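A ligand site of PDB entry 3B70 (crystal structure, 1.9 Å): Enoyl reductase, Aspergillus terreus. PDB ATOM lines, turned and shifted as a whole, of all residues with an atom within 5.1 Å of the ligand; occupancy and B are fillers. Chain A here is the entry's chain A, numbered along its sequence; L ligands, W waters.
The side-chain hydroxyl (OG) of Ser 197 lies within hydrogen-bond range of the guanidinium group (NH1) of Arg 216, 2.9 Å away. The backbone carbonyl oxygen (O) of Ser 174 sits at hydrogen-bond distance from a ring nitrogen (NE2) of His 327, at 3.0 Å. NZ of Lys 54 lies close to ND2 of Asn 263. OG1 of Thr 280 lies within hydrogen-bond range of O of Leu 262, 3.2 Å away. ND1 of His 199 sits at hydrogen-bond distance from OD1 of Asn 200 (3.5 Å). O of Tyr 171 sits at hydrogen-bond distance from N of Cys 238 (2.9 Å). N of Ala 178 is in hydrogen-bond range of OG1 of Thr 175 (3.0 Å). The side-chain hydroxyl (OH) of Tyr 215 is in hydrogen-bond range of the guanidinium group (NH2) of Arg 216 (3.1 Å).
Water W12 lies within hydrogen-bond range of OH of Tyr 215, O15 of the ligand and NH2 of Arg 216. Water W7 lies within hydrogen-bond range of O9 of the ligand (2.7 Å) and NZ of Lys 355 (2.8 Å). Water W15 lies within hydrogen-bond range of O1 of the ligand (2.7 Å), O of Ser 174 (3.0 Å), N of Gly 353 (3.2 Å) and N of Glu 354 (3.4 Å). Water W14 bridges OD1 of Asn 49 (2.6 Å) and O9 of the ligand (2.8 Å). Water W1 bridges the backbone carbonyl oxygen of Thr 280 (3.1 Å) and a nitrogen (N7) of the ligand (3.2 Å). Water W13 lies within hydrogen-bond range of a nitrogen (N3) of the ligand (3.2 Å) and the side-chain amide nitrogen of Asn 241 (3.3 Å).
O16 of the ligand is in hydrogen-bond range of N of Ser 197 (3.0 Å). O15 of the ligand sits at hydrogen-bond distance from OG of Ser 197 (2.5 Å). The backbone NH of Thr 177 is in hydrogen-bond range of an oxygen (O8) of the ligand, 2.9 Å away. OG1 of Thr 177 is in hydrogen-bond range of O8 of the ligand (2.6 Å). OG of Ser 174 sits at hydrogen-bond distance from O16 of the ligand. O13 of the ligand lies within hydrogen-bond range of NZ of Lys 54, at 2.7 Å. O17 of the ligand is in hydrogen-bond range of OG of Ser 352 (2.7 Å). A nitrogen (N7) of the ligand sits at hydrogen-bond distance from the backbone carbonyl oxygen (O) of Leu 262 (2.7 Å). ND2 of Asn 200 is in hydrogen-bond range of O16 of the ligand, at 2.8 Å. ND2 of Asn 263 sits at hydrogen-bond distance from O12 of the ligand (2.9 Å). N of Ala 176 is in hydrogen-bond range of O1 of the ligand (3.1 Å). A nitrogen (N7) of the ligand sits at hydrogen-bond distance from the backbone carbonyl oxygen (O) of Thr 280 (3.2 Å). OG of Ser 51 sits at hydrogen-bond distance from O13 of the ligand, at 3.3 Å. The side-chain amide nitrogen of Asn 241 sits close to a nitrogen (N3) of the ligand, at 3.4 Å. N of Gly 353 is in hydrogen-bond range of O5 of the ligand, at 3.5 Å.
Merely in contact with the ligand: Pro 50 (3.3 Å), Thr 139 (3.2 Å), Thr 175 (3.3 Å), Cys 196 (3.6 Å), His 199 (3.6 Å), Tyr 215 (3.4 Å), Cys 238 (3.2 Å), Ile 239 (3.5 Å), Gly 282 (3.3 Å) and Leu 351 (3.8 Å). Hydrophobic or aromatic side chains that line the ligand: Pro 50, Ala 176, Tyr 215, Ile 239 and Leu 262. Within 4 Å of the ligand: Pro 50, Ser 51, Lys 54, Thr 139, Ser 174, Thr 175, Ala 176, Thr 177, Cys 196, Ser 197, His 199, Asn 200, Tyr 215, Cys 238, Ile 239, Asn 241, Leu 262, Asn 263, Thr 280, Gly 282, Leu 351, Ser 352 and Gly 353. The nearest printed residue that does not touch the ligand is Tyr 171 (4.1 Å).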
ATOM      1  N   ASN A  49     -27.569  32.641  12.809  1.00  0.00           N
ATOM      2  CA  ASN A  49     -27.267  31.720  11.718  1.00  0.00           C
ATOM      3  C   ASN A  49     -25.802  31.390  11.692  1.00  0.00           C
ATOM      4  O   ASN A  49     -24.985  32.266  12.012  1.00  0.00           O
ATOM      5  CB  ASN A  49     -27.666  32.344  10.373  1.00  0.00           C
ATOM      6  CG  ASN A  49     -29.160  32.350  10.189  1.00  0.00           C
ATOM      7  OD1 ASN A  49     -29.762  31.343   9.799  1.00  0.00           O
ATOM      8  ND2 ASN A  49     -29.774  33.492  10.465  1.00  0.00           N
ATOM      9  N   PRO A  50     -25.421  30.165  11.270  1.00  0.00           N
ATOM     10  CA  PRO A  50     -23.979  29.861  11.131  1.00  0.00           C
ATOM     11  C   PRO A  50     -23.237  30.874  10.284  1.00  0.00           C
ATOM     12  O   PRO A  50     -22.059  31.215  10.552  1.00  0.00           O
ATOM     13  CB  PRO A  50     -23.971  28.455  10.470  1.00  0.00           C
ATOM     14  CG  PRO A  50     -25.194  27.846  10.898  1.00  0.00           C
ATOM     15  CD  PRO A  50     -26.248  28.986  10.961  1.00  0.00           C
ATOM     16  N   SER A  51     -23.879  31.376   9.240  1.00  0.00           N
ATOM     17  CA  SER A  51     -23.207  32.344   8.394  1.00  0.00           C
ATOM     18  C   SER A  51     -22.764  33.631   9.141  1.00  0.00           C
ATOM     19  O   SER A  51     -21.686  34.181   8.827  1.00  0.00           O
ATOM     20  CB  SER A  51     -23.984  32.561   7.083  1.00  0.00           C
ATOM     21  OG  SER A  51     -24.037  31.274   6.410  1.00  0.00           O
ATOM     22  N   LYS A  54     -19.331  33.095  10.664  1.00  0.00           N
ATOM     23  CA  LYS A  54     -18.225  32.991   9.712  1.00  0.00           C
ATOM     24  C   LYS A  54     -17.736  34.343   9.192  1.00  0.00           C
ATOM     25  O   LYS A  54     -16.807  34.399   8.370  1.00  0.00           O
ATOM     26  CB  LYS A  54     -18.598  32.060   8.539  1.00  0.00           C
ATOM     27  CG  LYS A  54     -18.920  30.612   8.958  1.00  0.00           C
ATOM     28  CD  LYS A  54     -19.653  29.900   7.820  1.00  0.00           C
ATOM     29  CE  LYS A  54     -20.019  28.483   8.180  1.00  0.00           C
ATOM     30  NZ  LYS A  54     -20.568  27.878   6.947  1.00  0.00           N
ATOM     31  N   THR A 139     -32.952  30.702   1.642  1.00  0.00           N
ATOM     32  CA  THR A 139     -32.067  29.614   1.204  1.00  0.00           C
ATOM     33  C   THR A 139     -32.804  28.457   0.534  1.00  0.00           C
ATOM     34  O   THR A 139     -32.299  27.887  -0.458  1.00  0.00           O
ATOM     35  CB  THR A 139     -31.208  29.106   2.390  1.00  0.00           C
ATOM     36  OG1 THR A 139     -30.600  30.218   3.056  1.00  0.00           O
ATOM     37  CG2 THR A 139     -30.115  28.195   1.856  1.00  0.00           C
ATOM     38  N   TYR A 171     -29.161  15.975   2.653  1.00  0.00           N
ATOM     39  CA  TYR A 171     -28.141  15.564   3.610  1.00  0.00           C
ATOM     40  C   TYR A 171     -28.091  16.603   4.722  1.00  0.00           C
ATOM     41  O   TYR A 171     -27.759  17.766   4.454  1.00  0.00           O
ATOM     42  CB  TYR A 171     -26.781  15.427   2.918  1.00  0.00           C
ATOM     43  CG  TYR A 171     -25.750  14.712   3.757  1.00  0.00           C
ATOM     44  CD1 TYR A 171     -25.544  13.333   3.618  1.00  0.00           C
ATOM     45  CD2 TYR A 171     -24.994  15.416   4.722  1.00  0.00           C
ATOM     46  CE1 TYR A 171     -24.612  12.632   4.419  1.00  0.00           C
ATOM     47  CE2 TYR A 171     -24.059  14.743   5.538  1.00  0.00           C
ATOM     48  CZ  TYR A 171     -23.869  13.350   5.361  1.00  0.00           C
ATOM     49  OH  TYR A 171     -22.933  12.720   6.136  1.00  0.00           O
ATOM     50  N   SER A 174     -31.966  17.779   9.712  1.00  0.00           N
ATOM     51  CA  SER A 174     -32.424  18.524  10.881  1.00  0.00           C
ATOM     52  C   SER A 174     -31.858  19.971  10.901  1.00  0.00           C
ATOM     53  O   SER A 174     -32.081  20.701  11.901  1.00  0.00           O
ATOM     54  CB  SER A 174     -31.982  17.837  12.190  1.00  0.00           C
ATOM     55  OG  SER A 174     -30.565  17.852  12.263  1.00  0.00           O
ATOM     56  N   THR A 175     -31.100  20.348   9.872  1.00  0.00           N
ATOM     57  CA  THR A 175     -30.586  21.732   9.769  1.00  0.00           C
ATOM     58  C   THR A 175     -31.764  22.690   9.618  1.00  0.00           C
ATOM     59  O   THR A 175     -32.837  22.332   9.048  1.00  0.00           O
ATOM     60  CB  THR A 175     -29.629  21.930   8.573  1.00  0.00           C
ATOM     61  OG1 THR A 175     -30.316  21.656   7.340  1.00  0.00           O
ATOM     62  CG2 THR A 175     -28.455  20.954   8.678  1.00  0.00           C
ATOM     63  N   ALA A 176     -31.592  23.902  10.141  1.00  0.00           N
ATOM     64  CA  ALA A 176     -32.606  24.959   9.966  1.00  0.00           C
ATOM     65  C   ALA A 176     -33.012  25.076   8.461  1.00  0.00           C
ATOM     66  O   ALA A 176     -34.205  25.207   8.100  1.00  0.00           O
ATOM     67  CB  ALA A 176     -32.042  26.283  10.483  1.00  0.00           C
ATOM     68  N   THR A 177     -32.042  25.005   7.568  1.00  0.00           N
ATOM     69  CA  THR A 177     -32.360  25.172   6.132  1.00  0.00           C
ATOM     70  C   THR A 177     -33.225  23.966   5.688  1.00  0.00           C
ATOM     71  O   THR A 177     -34.269  24.129   5.027  1.00  0.00           O
ATOM     72  CB  THR A 177     -31.086  25.317   5.265  1.00  0.00           C
ATOM     73  OG1 THR A 177     -30.298  26.434   5.767  1.00  0.00           O
ATOM     74  CG2 THR A 177     -31.409  25.494   3.709  1.00  0.00           C
ATOM     75  N   ALA A 178     -32.822  22.756   6.034  1.00  0.00           N
ATOM     76  CA  ALA A 178     -33.537  21.568   5.502  1.00  0.00           C
ATOM     77  C   ALA A 178     -34.958  21.483   5.972  1.00  0.00           C
ATOM     78  O   ALA A 178     -35.790  20.974   5.266  1.00  0.00           O
ATOM     79  CB  ALA A 178     -32.838  20.270   5.886  1.00  0.00           C
ATOM     80  N   CYS A 196     -29.800  12.451   9.109  1.00  0.00           N
ATOM     81  CA  CYS A 196     -29.481  13.306  10.244  1.00  0.00           C
ATOM     82  C   CYS A 196     -29.242  12.379  11.441  1.00  0.00           C
ATOM     83  O   CYS A 196     -29.143  11.162  11.250  1.00  0.00           O
ATOM     84  CB  CYS A 196     -30.642  14.278  10.529  1.00  0.00           C
ATOM     85  SG  CYS A 196     -32.241  13.544  11.075  1.00  0.00           S
ATOM     86  N   SER A 197     -29.175  12.926  12.659  1.00  0.00           N
ATOM     87  CA  SER A 197     -28.950  12.036  13.835  1.00  0.00           C
ATOM     88  C   SER A 197     -30.282  11.477  14.328  1.00  0.00           C
ATOM     89  O   SER A 197     -31.328  12.152  14.196  1.00  0.00           O
ATOM     90  CB  SER A 197     -28.217  12.748  14.972  1.00  0.00           C
ATOM     91  OG  SER A 197     -26.892  13.127  14.585  1.00  0.00           O
ATOM     92  N   HIS A 199     -31.879  11.297  17.061  1.00  0.00           N
ATOM     93  CA  HIS A 199     -32.752  12.092  17.956  1.00  0.00           C
ATOM     94  C   HIS A 199     -33.593  13.158  17.210  1.00  0.00           C
ATOM     95  O   HIS A 199     -34.604  13.633  17.728  1.00  0.00           O
ATOM     96  CB  HIS A 199     -31.974  12.701  19.111  1.00  0.00           C
ATOM     97  CG  HIS A 199     -31.040  13.810  18.725  1.00  0.00           C
ATOM     98  ND1 HIS A 199     -31.401  15.146  18.813  1.00  0.00           N
ATOM     99  CD2 HIS A 199     -29.772  13.791  18.270  1.00  0.00           C
ATOM    100  CE1 HIS A 199     -30.378  15.890  18.437  1.00  0.00           C
ATOM    101  NE2 HIS A 199     -29.378  15.100  18.103  1.00  0.00           N
ATOM    102  N   ASN A 200     -33.187  13.479  15.989  1.00  0.00           N
ATOM    103  CA  ASN A 200     -33.980  14.359  15.134  1.00  0.00           C
ATOM    104  C   ASN A 200     -34.858  13.693  14.054  1.00  0.00           C
ATOM    105  O   ASN A 200     -35.370  14.392  13.153  1.00  0.00           O
ATOM    106  CB  ASN A 200     -33.060  15.412  14.491  1.00  0.00           C
ATOM    107  CG  ASN A 200     -32.509  16.390  15.526  1.00  0.00           C
ATOM    108  OD1 ASN A 200     -33.235  16.847  16.399  1.00  0.00           O
ATOM    109  ND2 ASN A 200     -31.239  16.721  15.426  1.00  0.00           N
ATOM    110  N   TYR A 215     -26.847   9.347   9.194  1.00  0.00           N
ATOM    111  CA  TYR A 215     -25.763   9.485   8.214  1.00  0.00           C
ATOM    112  C   TYR A 215     -24.497   8.633   8.530  1.00  0.00           C
ATOM    113  O   TYR A 215     -23.629   8.430   7.658  1.00  0.00           O
ATOM    114  CB  TYR A 215     -25.409  10.968   8.003  1.00  0.00           C
ATOM    115  CG  TYR A 215     -24.768  11.597   9.236  1.00  0.00           C
ATOM    116  CD1 TYR A 215     -23.366  11.593   9.382  1.00  0.00           C
ATOM    117  CD2 TYR A 215     -25.537  12.213  10.187  1.00  0.00           C
ATOM    118  CE1 TYR A 215     -22.771  12.166  10.519  1.00  0.00           C
ATOM    119  CE2 TYR A 215     -24.969  12.798  11.333  1.00  0.00           C
ATOM    120  CZ  TYR A 215     -23.587  12.757  11.470  1.00  0.00           C
ATOM    121  OH  TYR A 215     -23.017  13.349  12.554  1.00  0.00           O
ATOM    122  N   ARG A 216     -24.366   8.226   9.793  1.00  0.00           N
ATOM    123  CA  ARG A 216     -23.235   7.415  10.263  1.00  0.00           C
ATOM    124  C   ARG A 216     -23.412   5.914   9.872  1.00  0.00           C
ATOM    125  O   ARG A 216     -22.459   5.138   9.986  1.00  0.00           O
ATOM    126  CB  ARG A 216     -23.118   7.518  11.776  1.00  0.00           C
ATOM    127  CG  ARG A 216     -23.018   8.949  12.338  1.00  0.00           C
ATOM    128  CD  ARG A 216     -23.172   8.911  13.874  1.00  0.00           C
ATOM    129  NE  ARG A 216     -23.110  10.228  14.507  1.00  0.00           N
ATOM    130  CZ  ARG A 216     -24.169  11.033  14.626  1.00  0.00           C
ATOM    131  NH1 ARG A 216     -25.354  10.686  14.087  1.00  0.00           N
ATOM    132  NH2 ARG A 216     -24.046  12.207  15.270  1.00  0.00           N
ATOM    133  N   CYS A 238     -26.810  20.123   3.013  1.00  0.00           N
ATOM    134  CA  CYS A 238     -26.965  21.193   3.990  1.00  0.00           C
ATOM    135  C   CYS A 238     -25.844  21.238   4.985  1.00  0.00           C
ATOM    136  O   CYS A 238     -25.884  22.051   5.888  1.00  0.00           O
ATOM    137  CB  CYS A 238     -28.293  21.043   4.704  1.00  0.00           C
ATOM    138  SG  CYS A 238     -29.759  21.211   3.670  1.00  0.00           S
ATOM    139  N   ILE A 239     -24.833  20.383   4.814  1.00  0.00           N
ATOM    140  CA  ILE A 239     -23.664  20.307   5.698  1.00  0.00           C
ATOM    141  C   ILE A 239     -22.432  20.853   4.996  1.00  0.00           C
ATOM    142  O   ILE A 239     -21.729  21.746   5.546  1.00  0.00           O
ATOM    143  CB  ILE A 239     -23.474  18.844   6.188  1.00  0.00           C
ATOM    144  CG1 ILE A 239     -24.769  18.363   6.899  1.00  0.00           C
ATOM    145  CG2 ILE A 239     -22.144  18.671   6.988  1.00  0.00           C
ATOM    146  CD1 ILE A 239     -25.231  19.257   8.105  1.00  0.00           C
ATOM    147  N   ASN A 241     -19.200  19.317   3.738  1.00  0.00           N
ATOM    148  CA  ASN A 241     -17.818  19.011   4.097  1.00  0.00           C
ATOM    149  C   ASN A 241     -17.392  17.854   3.237  1.00  0.00           C
ATOM    150  O   ASN A 241     -18.163  17.399   2.359  1.00  0.00           O
ATOM    151  CB  ASN A 241     -17.655  18.734   5.610  1.00  0.00           C
ATOM    152  CG  ASN A 241     -18.553  17.599   6.115  1.00  0.00           C
ATOM    153  OD1 ASN A 241     -18.898  16.704   5.371  1.00  0.00           O
ATOM    154  ND2 ASN A 241     -18.934  17.645   7.365  1.00  0.00           N
ATOM    155  N   LEU A 262     -24.948  24.202   0.289  1.00  0.00           N
ATOM    156  CA  LEU A 262     -25.291  25.564   0.832  1.00  0.00           C
ATOM    157  C   LEU A 262     -24.028  26.441   0.988  1.00  0.00           C
ATOM    158  O   LEU A 262     -24.119  27.660   1.214  1.00  0.00           O
ATOM    159  CB  LEU A 262     -26.015  25.424   2.173  1.00  0.00           C
ATOM    160  CG  LEU A 262     -27.343  24.677   2.092  1.00  0.00           C
ATOM    161  CD1 LEU A 262     -28.020  24.664   3.452  1.00  0.00           C
ATOM    162  CD2 LEU A 262     -28.305  25.249   0.937  1.00  0.00           C
ATOM    163  N   ASN A 263     -22.864  25.792   0.938  1.00  0.00           N
ATOM    164  CA  ASN A 263     -21.547  26.482   1.006  1.00  0.00           C
ATOM    165  C   ASN A 263     -20.739  26.057  -0.244  1.00  0.00           C
ATOM    166  O   ASN A 263     -21.065  25.003  -0.832  1.00  0.00           O
ATOM    167  CB  ASN A 263     -20.772  26.056   2.275  1.00  0.00           C
ATOM    168  CG  ASN A 263     -21.450  26.509   3.621  1.00  0.00           C
ATOM    169  OD1 ASN A 263     -21.879  27.626   3.738  1.00  0.00           O
ATOM    170  ND2 ASN A 263     -21.453  25.619   4.644  1.00  0.00           N
ATOM    171  N   THR A 280     -25.405  27.698  -3.195  1.00  0.00           N
ATOM    172  CA  THR A 280     -26.196  28.878  -2.951  1.00  0.00           C
ATOM    173  C   THR A 280     -25.315  30.049  -2.471  1.00  0.00           C
ATOM    174  O   THR A 280     -24.578  29.914  -1.476  1.00  0.00           O
ATOM    175  CB  THR A 280     -27.274  28.634  -1.893  1.00  0.00           C
ATOM    176  OG1 THR A 280     -26.628  28.141  -0.704  1.00  0.00           O
ATOM    177  CG2 THR A 280     -28.330  27.626  -2.384  1.00  0.00           C
ATOM    178  N   LEU A 281     -25.446  31.191  -3.142  1.00  0.00           N
ATOM    179  CA  LEU A 281     -24.762  32.425  -2.719  1.00  0.00           C
ATOM    180  C   LEU A 281     -25.826  33.335  -2.087  1.00  0.00           C
ATOM    181  O   LEU A 281     -26.737  33.845  -2.740  1.00  0.00           O
ATOM    182  CB  LEU A 281     -24.060  33.093  -3.923  1.00  0.00           C
ATOM    183  CG  LEU A 281     -23.308  34.443  -3.666  1.00  0.00           C
ATOM    184  CD1 LEU A 281     -22.265  34.336  -2.561  1.00  0.00           C
ATOM    185  CD2 LEU A 281     -22.689  34.949  -4.993  1.00  0.00           C
ATOM    186  N   GLY A 282     -25.711  33.485  -0.777  1.00  0.00           N
ATOM    187  CA  GLY A 282     -26.803  34.059   0.025  1.00  0.00           C
ATOM    188  C   GLY A 282     -27.243  35.443  -0.433  1.00  0.00           C
ATOM    189  O   GLY A 282     -28.439  35.666  -0.610  1.00  0.00           O
ATOM    190  N   HIS A 327     -38.486  26.497  12.125  1.00  0.00           N
ATOM    191  CA  HIS A 327     -37.644  25.477  12.755  1.00  0.00           C
ATOM    192  C   HIS A 327     -37.920  25.566  14.280  1.00  0.00           C
ATOM    193  O   HIS A 327     -38.313  26.653  14.746  1.00  0.00           O
ATOM    194  CB  HIS A 327     -36.186  25.807  12.431  1.00  0.00           C
ATOM    195  CG  HIS A 327     -35.272  24.627  12.528  1.00  0.00           C
ATOM    196  ND1 HIS A 327     -34.164  24.612  13.341  1.00  0.00           N
ATOM    197  CD2 HIS A 327     -35.277  23.442  11.874  1.00  0.00           C
ATOM    198  CE1 HIS A 327     -33.532  23.460  13.191  1.00  0.00           C
ATOM    199  NE2 HIS A 327     -34.184  22.735  12.309  1.00  0.00           N
ATOM    200  N   LEU A 351     -25.907  23.535  18.850  1.00  0.00           N
ATOM    201  CA  LEU A 351     -27.347  23.446  18.696  1.00  0.00           C
ATOM    202  C   LEU A 351     -27.654  22.267  17.767  1.00  0.00           C
ATOM    203  O   LEU A 351     -26.938  22.058  16.759  1.00  0.00           O
ATOM    204  CB  LEU A 351     -27.936  24.741  18.131  1.00  0.00           C
ATOM    205  CG  LEU A 351     -27.969  26.066  18.927  1.00  0.00           C
ATOM    206  CD1 LEU A 351     -28.539  27.126  17.996  1.00  0.00           C
ATOM    207  CD2 LEU A 351     -28.812  25.992  20.168  1.00  0.00           C
ATOM    208  N   SER A 352     -28.676  21.499  18.104  1.00  0.00           N
ATOM    209  CA  SER A 352     -29.179  20.438  17.252  1.00  0.00           C
ATOM    210  C   SER A 352     -30.712  20.473  17.223  1.00  0.00           C
ATOM    211  O   SER A 352     -31.383  20.467  18.262  1.00  0.00           O
ATOM    212  CB  SER A 352     -28.665  19.057  17.733  1.00  0.00           C
ATOM    213  OG  SER A 352     -29.246  18.041  16.965  1.00  0.00           O
ATOM    214  N   GLY A 353     -31.260  20.570  16.021  1.00  0.00           N
ATOM    215  CA  GLY A 353     -32.694  20.559  15.780  1.00  0.00           C
ATOM    216  C   GLY A 353     -33.406  21.767  16.344  1.00  0.00           C
ATOM    217  O   GLY A 353     -34.592  21.694  16.609  1.00  0.00           O
ATOM    218  N   GLU A 354     -32.676  22.872  16.511  1.00  0.00           N
ATOM    219  CA  GLU A 354     -33.234  24.108  17.093  1.00  0.00           C
ATOM    220  C   GLU A 354     -32.599  25.322  16.488  1.00  0.00           C
ATOM    221  O   GLU A 354     -31.427  25.279  16.100  1.00  0.00           O
ATOM    222  CB  GLU A 354     -32.884  24.185  18.574  1.00  0.00           C
ATOM    223  CG  GLU A 354     -33.452  23.118  19.419  1.00  0.00           C
ATOM    224  CD  GLU A 354     -33.098  23.303  20.856  1.00  0.00           C
ATOM    225  OE1 GLU A 354     -31.895  23.354  21.201  1.00  0.00           O
ATOM    226  OE2 GLU A 354     -34.042  23.442  21.633  1.00  0.00           O
ATOM    227  N   LYS A 355     -33.347  26.417  16.465  1.00  0.00           N
ATOM    228  CA  LYS A 355     -32.866  27.725  16.003  1.00  0.00           C
ATOM    229  C   LYS A 355     -32.737  28.661  17.216  1.00  0.00           C
ATOM    230  O   LYS A 355     -33.706  28.831  17.922  1.00  0.00           O
ATOM    231  CB  LYS A 355     -33.932  28.329  15.094  1.00  0.00           C
ATOM    232  CG  LYS A 355     -33.504  29.572  14.302  1.00  0.00           C
ATOM    233  CD  LYS A 355     -32.629  29.161  13.111  1.00  0.00           C
ATOM    234  CE  LYS A 355     -32.295  30.342  12.248  1.00  0.00           C
ATOM    235  NZ  LYS A 355     -31.300  29.874  11.213  1.00  0.00           N
HETATM  236  P1  LIG L   1     -28.044  24.342  11.518  1.00  0.00           P
HETATM  237  O1  LIG L   1     -29.341  24.441  12.164  1.00  0.00           O
HETATM  238  O2  LIG L   1     -26.966  25.182  12.002  1.00  0.00           O
HETATM  239  O3  LIG L   1     -27.495  22.805  11.463  1.00  0.00           O
HETATM  240  C1  LIG L   1     -27.094  22.149  12.646  1.00  0.00           C
HETATM  241  C2  LIG L   1     -27.189  20.635  12.356  1.00  0.00           C
HETATM  242  O4  LIG L   1     -26.152  20.145  11.505  1.00  0.00           O
HETATM  243  C3  LIG L   1     -27.128  19.832  13.663  1.00  0.00           C
HETATM  244  O5  LIG L   1     -28.468  19.667  14.117  1.00  0.00           O
HETATM  245  C4  LIG L   1     -26.579  18.485  13.177  1.00  0.00           C
HETATM  246  O6  LIG L   1     -27.692  17.660  12.953  1.00  0.00           O
HETATM  247  C5  LIG L   1     -25.984  18.728  11.803  1.00  0.00           C
HETATM  248  N1  LIG L   1     -24.569  18.484  11.675  1.00  0.00           N
HETATM  249  C6  LIG L   1     -23.558  19.309  12.138  1.00  0.00           C
HETATM  250  N2  LIG L   1     -22.386  18.784  11.731  1.00  0.00           N
HETATM  251  C7  LIG L   1     -22.635  17.678  10.965  1.00  0.00           C
HETATM  252  C8  LIG L   1     -21.797  16.765  10.305  1.00  0.00           C
HETATM  253  N3  LIG L   1     -20.473  16.907  10.310  1.00  0.00           N
HETATM  254  N4  LIG L   1     -22.391  15.747   9.569  1.00  0.00           N
HETATM  255  C9  LIG L   1     -23.760  15.567   9.581  1.00  0.00           C
HETATM  256  N5  LIG L   1     -24.590  16.460  10.237  1.00  0.00           N
HETATM  257  C10 LIG L   1     -24.008  17.510  10.908  1.00  0.00           C
HETATM  258  O7  LIG L   1     -28.182  24.563   9.919  1.00  0.00           O
HETATM  259  P2  LIG L   1     -28.248  25.816   8.913  1.00  0.00           P
HETATM  260  O8  LIG L   1     -29.201  25.397   7.865  1.00  0.00           O
HETATM  261  O9  LIG L   1     -28.503  27.018   9.689  1.00  0.00           O
HETATM  262  O10 LIG L   1     -26.776  25.882   8.314  1.00  0.00           O
HETATM  263  C11 LIG L   1     -26.240  24.704   7.713  1.00  0.00           C
HETATM  264  C12 LIG L   1     -25.033  25.040   6.854  1.00  0.00           C
HETATM  265  O11 LIG L   1     -25.474  25.709   5.675  1.00  0.00           O
HETATM  266  C13 LIG L   1     -24.077  25.991   7.576  1.00  0.00           C
HETATM  267  O12 LIG L   1     -22.777  25.645   7.198  1.00  0.00           O
HETATM  268  C14 LIG L   1     -24.397  27.330   6.946  1.00  0.00           C
HETATM  269  O13 LIG L   1     -23.245  28.158   6.956  1.00  0.00           O
HETATM  270  C15 LIG L   1     -24.833  26.927   5.533  1.00  0.00           C
HETATM  271  N6  LIG L   1     -25.809  27.895   5.027  1.00  0.00           N
HETATM  272  C16 LIG L   1     -25.388  28.778   4.083  1.00  0.00           C
HETATM  273  C17 LIG L   1     -26.281  29.705   3.596  1.00  0.00           C
HETATM  274  C18 LIG L   1     -25.805  30.616   2.495  1.00  0.00           C
HETATM  275  O14 LIG L   1     -26.445  31.835   2.378  1.00  0.00           O
HETATM  276  N7  LIG L   1     -24.800  30.263   1.688  1.00  0.00           N
HETATM  277  C19 LIG L   1     -27.595  29.795   4.092  1.00  0.00           C
HETATM  278  C20 LIG L   1     -27.989  28.885   5.082  1.00  0.00           C
HETATM  279  C21 LIG L   1     -27.077  27.948   5.540  1.00  0.00           C
HETATM  280  P3  LIG L   1     -27.936  16.268  13.773  1.00  0.00           P
HETATM  281  O15 LIG L   1     -26.876  15.307  13.280  1.00  0.00           O
HETATM  282  O16 LIG L   1     -29.371  15.836  13.535  1.00  0.00           O
HETATM  283  O17 LIG L   1     -27.740  16.624  15.232  1.00  0.00           O
HETATM  284  O   HOH W   1     -22.017  30.483   0.206  1.00  0.00           O
HETATM  285  O   HOH W   2     -26.266  30.511   7.662  1.00  0.00           O
HETATM  286  O   HOH W   3     -21.274  14.370   7.515  1.00  0.00           O
HETATM  287  O   HOH W   4     -25.463  17.369  16.431  1.00  0.00           O
HETATM  288  O   HOH W   5     -29.020  17.439  10.094  1.00  0.00           O
HETATM  289  O   HOH W   6     -23.309  32.751   0.824  1.00  0.00           O
HETATM  290  O   HOH W   7     -29.445  27.938  12.049  1.00  0.00           O
HETATM  291  O   HOH W   8     -23.705  22.281  13.795  1.00  0.00           O
HETATM  292  O   HOH W   9     -26.746  25.529  14.745  1.00  0.00           O
HETATM  293  O   HOH W  10     -29.675  26.386  14.341  1.00  0.00           O
HETATM  294  O   HOH W  11     -27.145  15.560  10.462  1.00  0.00           O
HETATM  295  O   HOH W  12     -24.237  15.351  13.803  1.00  0.00           O
HETATM  296  O   HOH W  13     -18.740  14.633   8.791  1.00  0.00           O
HETATM  297  O   HOH W  14     -28.943  29.364   8.317  1.00  0.00           O
HETATM  298  O   HOH W  15     -30.773  22.744  13.721  1.00  0.00           O
